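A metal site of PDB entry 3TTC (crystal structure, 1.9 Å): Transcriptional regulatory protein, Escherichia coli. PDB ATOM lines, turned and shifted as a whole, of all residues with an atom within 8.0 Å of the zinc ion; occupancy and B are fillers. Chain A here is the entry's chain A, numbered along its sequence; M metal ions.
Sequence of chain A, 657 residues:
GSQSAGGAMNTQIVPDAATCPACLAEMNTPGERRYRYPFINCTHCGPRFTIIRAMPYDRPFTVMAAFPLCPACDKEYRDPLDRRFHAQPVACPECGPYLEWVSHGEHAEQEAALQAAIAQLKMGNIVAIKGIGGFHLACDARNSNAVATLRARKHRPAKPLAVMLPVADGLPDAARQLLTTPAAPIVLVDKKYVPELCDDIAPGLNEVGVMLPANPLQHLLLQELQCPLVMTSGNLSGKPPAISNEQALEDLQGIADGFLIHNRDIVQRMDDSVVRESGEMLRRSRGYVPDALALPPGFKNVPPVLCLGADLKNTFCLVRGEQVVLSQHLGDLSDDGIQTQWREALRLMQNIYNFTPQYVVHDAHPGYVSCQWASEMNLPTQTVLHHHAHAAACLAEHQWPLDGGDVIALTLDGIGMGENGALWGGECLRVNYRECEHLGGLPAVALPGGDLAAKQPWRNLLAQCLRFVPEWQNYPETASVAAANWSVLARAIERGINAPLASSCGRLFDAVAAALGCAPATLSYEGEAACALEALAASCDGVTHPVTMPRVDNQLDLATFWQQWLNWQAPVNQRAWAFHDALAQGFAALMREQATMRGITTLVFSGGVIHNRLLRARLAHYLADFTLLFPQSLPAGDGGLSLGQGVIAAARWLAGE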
ATOM      1  N   ALA A  17       4.684   0.001   1.258  1.00  0.00           N
ATOM      2  CA  ALA A  17       5.479  -1.019   1.974  1.00  0.00           C
ATOM      3  C   ALA A  17       5.686  -2.257   1.143  1.00  0.00           C
ATOM      4  O   ALA A  17       4.732  -2.758   0.538  1.00  0.00           O
ATOM      5  CB  ALA A  17       4.796  -1.411   3.296  1.00  0.00           C
ATOM      6  N   ALA A  18       6.906  -2.771   1.144  1.00  0.00           N
ATOM      7  CA  ALA A  18       7.239  -4.038   0.469  1.00  0.00           C
ATOM      8  C   ALA A  18       6.289  -5.176   0.861  1.00  0.00           C
ATOM      9  O   ALA A  18       5.961  -5.314   2.038  1.00  0.00           O
ATOM     10  CB  ALA A  18       8.685  -4.443   0.806  1.00  0.00           C
ATOM     11  N   THR A  19       5.892  -6.013  -0.105  1.00  0.00           N
ATOM     12  CA  THR A  19       5.113  -7.242   0.192  1.00  0.00           C
ATOM     13  C   THR A  19       5.741  -8.001   1.380  1.00  0.00           C
ATOM     14  O   THR A  19       6.941  -8.240   1.414  1.00  0.00           O
ATOM     15  CB  THR A  19       5.087  -8.175  -1.062  1.00  0.00           C
ATOM     16  OG1 THR A  19       4.579  -7.418  -2.172  1.00  0.00           O
ATOM     17  CG2 THR A  19       4.203  -9.430  -0.819  1.00  0.00           C
ATOM     18  N   CYS A  20       4.907  -8.361   2.356  1.00  0.00           N
ATOM     19  CA  CYS A  20       5.389  -8.985   3.608  1.00  0.00           C
ATOM     20  C   CYS A  20       5.606 -10.481   3.403  1.00  0.00           C
ATOM     21  O   CYS A  20       5.116 -11.041   2.403  1.00  0.00           O
ATOM     22  CB  CYS A  20       4.376  -8.719   4.728  1.00  0.00           C
ATOM     23  SG  CYS A  20       2.828  -9.664   4.582  1.00  0.00           S
ATOM     24  N   PRO A  21       6.394 -11.124   4.284  1.00  0.00           N
ATOM     25  CA  PRO A  21       6.622 -12.593   4.162  1.00  0.00           C
ATOM     26  C   PRO A  21       5.332 -13.428   4.069  1.00  0.00           C
ATOM     27  O   PRO A  21       5.275 -14.398   3.309  1.00  0.00           O
ATOM     28  CB  PRO A  21       7.425 -12.949   5.421  1.00  0.00           C
ATOM     29  CG  PRO A  21       8.201 -11.661   5.735  1.00  0.00           C
ATOM     30  CD  PRO A  21       7.194 -10.535   5.380  1.00  0.00           C
ATOM     31  N   ALA A  22       4.317 -13.056   4.843  1.00  0.00           N
ATOM     32  CA  ALA A  22       3.051 -13.783   4.870  1.00  0.00           C
ATOM     33  C   ALA A  22       2.319 -13.692   3.528  1.00  0.00           C
ATOM     34  O   ALA A  22       1.760 -14.682   3.070  1.00  0.00           O
ATOM     35  CB  ALA A  22       2.171 -13.271   6.012  1.00  0.00           C
ATOM     36  N   CYS A  23       2.319 -12.520   2.897  1.00  0.00           N
ATOM     37  CA  CYS A  23       1.670 -12.391   1.593  1.00  0.00           C
ATOM     38  C   CYS A  23       2.473 -13.134   0.534  1.00  0.00           C
ATOM     39  O   CYS A  23       1.903 -13.792  -0.327  1.00  0.00           O
ATOM     40  CB  CYS A  23       1.483 -10.912   1.176  1.00  0.00           C
ATOM     41  SG  CYS A  23       0.102 -10.057   2.023  1.00  0.00           S
ATOM     42  N   LEU A  24       3.787 -13.030   0.604  1.00  0.00           N
ATOM     43  CA  LEU A  24       4.653 -13.794  -0.295  1.00  0.00           C
ATOM     44  C   LEU A  24       4.375 -15.314  -0.169  1.00  0.00           C
ATOM     45  O   LEU A  24       4.189 -15.986  -1.190  1.00  0.00           O
ATOM     46  CB  LEU A  24       6.115 -13.475  -0.036  1.00  0.00           C
ATOM     47  CG  LEU A  24       7.135 -14.090  -1.012  1.00  0.00           C
ATOM     48  CD1 LEU A  24       6.777 -13.765  -2.474  1.00  0.00           C
ATOM     49  CD2 LEU A  24       8.528 -13.572  -0.677  1.00  0.00           C
ATOM     50  N   GLU A  26       1.657 -16.772   0.926  1.00  0.00           N
ATOM     51  CA  GLU A  26       0.310 -16.976   0.360  1.00  0.00           C
ATOM     52  C   GLU A  26       0.333 -17.030  -1.178  1.00  0.00           C
ATOM     53  O   GLU A  26      -0.249 -17.941  -1.787  1.00  0.00           O
ATOM     54  CB  GLU A  26      -0.655 -15.893   0.852  1.00  0.00           C
ATOM     55  CG  GLU A  26      -2.126 -16.106   0.443  1.00  0.00           C
ATOM     56  CD  GLU A  26      -3.065 -14.991   0.933  1.00  0.00           C
ATOM     57  OE1 GLU A  26      -2.712 -14.231   1.869  1.00  0.00           O
ATOM     58  OE2 GLU A  26      -4.159 -14.872   0.362  1.00  0.00           O
ATOM     59  N   ILE A  40      -1.654  -9.070  -4.504  1.00  0.00           N
ATOM     60  CA  ILE A  40      -1.862  -9.468  -3.123  1.00  0.00           C
ATOM     61  C   ILE A  40      -1.274  -8.422  -2.151  1.00  0.00           C
ATOM     62  O   ILE A  40      -0.169  -7.881  -2.382  1.00  0.00           O
ATOM     63  CB  ILE A  40      -1.258 -10.889  -2.873  1.00  0.00           C
ATOM     64  CG1 ILE A  40      -1.527 -11.368  -1.447  1.00  0.00           C
ATOM     65  CG2 ILE A  40       0.271 -10.935  -3.200  1.00  0.00           C
ATOM     66  CD1 ILE A  40      -1.239 -12.859  -1.287  1.00  0.00           C
ATOM     67  N   ASN A  41      -2.032  -8.110  -1.097  1.00  0.00           N
ATOM     68  CA  ASN A  41      -1.546  -7.238  -0.022  1.00  0.00           C
ATOM     69  C   ASN A  41      -2.321  -7.531   1.248  1.00  0.00           C
ATOM     70  O   ASN A  41      -3.312  -8.266   1.210  1.00  0.00           O
ATOM     71  CB  ASN A  41      -1.583  -5.742  -0.415  1.00  0.00           C
ATOM     72  CG  ASN A  41      -2.956  -5.270  -0.862  1.00  0.00           C
ATOM     73  OD1 ASN A  41      -3.194  -5.051  -2.052  1.00  0.00           O
ATOM     74  ND2 ASN A  41      -3.857  -5.066   0.096  1.00  0.00           N
ATOM     75  N   CYS A  42      -1.873  -6.985   2.377  1.00  0.00           N
ATOM     76  CA  CYS A  42      -2.589  -7.194   3.633  1.00  0.00           C
ATOM     77  C   CYS A  42      -2.506  -5.928   4.482  1.00  0.00           C
ATOM     78  O   CYS A  42      -2.048  -4.898   4.001  1.00  0.00           O
ATOM     79  CB  CYS A  42      -2.022  -8.405   4.384  1.00  0.00           C
ATOM     80  SG  CYS A  42      -0.399  -8.125   5.140  1.00  0.00           S
ATOM     81  N   THR A  43      -2.937  -5.996   5.749  1.00  0.00           N
ATOM     82  CA  THR A  43      -2.874  -4.775   6.555  1.00  0.00           C
ATOM     83  C   THR A  43      -1.445  -4.262   6.770  1.00  0.00           C
ATOM     84  O   THR A  43      -1.236  -3.081   7.011  1.00  0.00           O
ATOM     85  CB  THR A  43      -3.657  -4.877   7.888  1.00  0.00           C
ATOM     86  OG1 THR A  43      -3.855  -3.561   8.418  1.00  0.00           O
ATOM     87  CG2 THR A  43      -2.914  -5.732   8.899  1.00  0.00           C
ATOM     88  N   HIS A  44      -0.462  -5.161   6.643  1.00  0.00           N
ATOM     89  CA  HIS A  44       0.937  -4.811   6.907  1.00  0.00           C
ATOM     90  C   HIS A  44       1.766  -4.401   5.681  1.00  0.00           C
ATOM     91  O   HIS A  44       2.898  -3.934   5.836  1.00  0.00           O
ATOM     92  CB  HIS A  44       1.638  -5.974   7.606  1.00  0.00           C
ATOM     93  CG  HIS A  44       0.947  -6.395   8.865  1.00  0.00           C
ATOM     94  ND1 HIS A  44       0.242  -7.578   8.958  1.00  0.00           N
ATOM     95  CD2 HIS A  44       0.831  -5.782  10.061  1.00  0.00           C
ATOM     96  CE1 HIS A  44      -0.265  -7.687  10.184  1.00  0.00           C
ATOM     97  NE2 HIS A  44       0.075  -6.608  10.869  1.00  0.00           N
ATOM     98  N   CYS A  45       1.244  -4.589   4.482  1.00  0.00           N
ATOM     99  CA  CYS A  45       2.040  -4.319   3.299  1.00  0.00           C
ATOM    100  C   CYS A  45       1.230  -3.806   2.120  1.00  0.00           C
ATOM    101  O   CYS A  45      -0.005  -3.838   2.135  1.00  0.00           O
ATOM    102  CB  CYS A  45       2.823  -5.583   2.874  1.00  0.00           C
ATOM    103  SG  CYS A  45       1.842  -6.854   2.027  1.00  0.00           S
ATOM    104  N   GLY A  46       1.941  -3.342   1.087  1.00  0.00           N
ATOM    105  CA  GLY A  46       1.306  -2.945  -0.169  1.00  0.00           C
ATOM    106  C   GLY A  46       1.297  -1.431  -0.393  1.00  0.00           C
ATOM    107  O   GLY A  46       1.835  -0.668   0.414  1.00  0.00           O
ATOM    108  N   ARG A  48       0.198   2.472  -0.552  1.00  0.00           N
ATOM    109  CA  ARG A  48      -0.536   3.329   0.383  1.00  0.00           C
ATOM    110  C   ARG A  48      -0.695   4.720  -0.255  1.00  0.00           C
ATOM    111  O   ARG A  48      -1.683   5.001  -0.931  1.00  0.00           O
ATOM    112  CB  ARG A  48       0.197   3.403   1.733  1.00  0.00           C
ATOM    113  CG  ARG A  48       0.300   2.047   2.488  1.00  0.00           C
ATOM    114  CD  ARG A  48      -1.042   1.657   3.120  1.00  0.00           C
ATOM    115  NE  ARG A  48      -0.934   0.421   3.897  1.00  0.00           N
ATOM    116  CZ  ARG A  48      -1.062  -0.807   3.390  1.00  0.00           C
ATOM    117  NH1 ARG A  48      -0.952  -1.846   4.209  1.00  0.00           N
ATOM    118  NH2 ARG A  48      -1.280  -0.994   2.090  1.00  0.00           N
ATOM    119  N   ARG A  83      -5.417 -11.185   8.821  1.00  0.00           N
ATOM    120  CA  ARG A  83      -4.284 -10.334   8.434  1.00  0.00           C
ATOM    121  C   ARG A  83      -4.672  -9.271   7.406  1.00  0.00           C
ATOM    122  O   ARG A  83      -3.995  -8.251   7.281  1.00  0.00           O
ATOM    123  CB  ARG A  83      -3.130 -11.186   7.899  1.00  0.00           C
ATOM    124  CG  ARG A  83      -1.801 -10.443   7.779  1.00  0.00           C
ATOM    125  CD  ARG A  83      -0.698 -11.303   7.191  1.00  0.00           C
ATOM    126  NE  ARG A  83      -0.762 -11.417   5.736  1.00  0.00           N
ATOM    127  CZ  ARG A  83      -1.192 -12.476   5.060  1.00  0.00           C
ATOM    128  NH1 ARG A  83      -1.634 -13.549   5.687  1.00  0.00           N
ATOM    129  NH2 ARG A  83      -1.195 -12.455   3.730  1.00  0.00           N
ATOM    130  N   ARG A  84      -5.761  -9.506   6.663  1.00  0.00           N
ATOM    131  CA  ARG A  84      -6.299  -8.549   5.694  1.00  0.00           C
ATOM    132  C   ARG A  84      -7.448  -7.678   6.210  1.00  0.00           C
ATOM    133  O   ARG A  84      -8.164  -7.048   5.415  1.00  0.00           O
ATOM    134  CB  ARG A  84      -6.721  -9.271   4.407  1.00  0.00           C
ATOM    135  CG  ARG A  84      -5.578  -9.993   3.765  1.00  0.00           C
ATOM    136  CD  ARG A  84      -6.068 -11.099   2.891  1.00  0.00           C
ATOM    137  NE  ARG A  84      -5.263 -12.304   3.083  1.00  0.00           N
ATOM    138  CZ  ARG A  84      -5.569 -13.301   3.927  1.00  0.00           C
ATOM    139  NH1 ARG A  84      -6.656 -13.238   4.681  1.00  0.00           N
ATOM    140  NH2 ARG A  84      -4.778 -14.354   4.005  1.00  0.00           N
ATOM    141  N   ALA A  87      -7.654  -4.074   5.053  1.00  0.00           N
ATOM    142  CA  ALA A  87      -6.611  -3.858   4.051  1.00  0.00           C
ATOM    143  C   ALA A  87      -7.330  -3.199   2.870  1.00  0.00           C
ATOM    144  O   ALA A  87      -7.980  -3.864   2.065  1.00  0.00           O
ATOM    145  CB  ALA A  87      -5.975  -5.173   3.639  1.00  0.00           C
HETATM  146 ZN    ZN M   1       1.150  -8.561   3.444  1.00  0.00          ZN
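SG of Cys 20 lies close to N of Ala 22, 3.7 Å away.
NH2 of Arg 83 sits close to SG of Cys 23, 3.2 Å away.
The backbone carbonyl oxygen (O) of Cys 45 is in hydrogen-bond range of the guanidinium group (NH1) of Arg 48, at 3.0 Å.
NE of Arg 83 sits close to SG of Cys 42 (3.4 Å).
The side-chain sulfur (SG) of Cys 42 sits close to the backbone NH (N) of His 44.
NH1 of Arg 48 lies within hydrogen-bond range of O of Cys 42 (3.2 Å).
The zinc ion is bound by the side-chain sulfur (SG) of Cys 20 (2.3 Å).
The zinc ion is bound by the side-chain sulfur (SG) of Cys 23.
The zinc ion is bound by the side-chain sulfur (SG) of Cys 45, 2.3 Å away.
The zinc ion is bound by SG of Cys 42 (2.3 Å).
The zinc ion has four donor atoms within binding distance.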
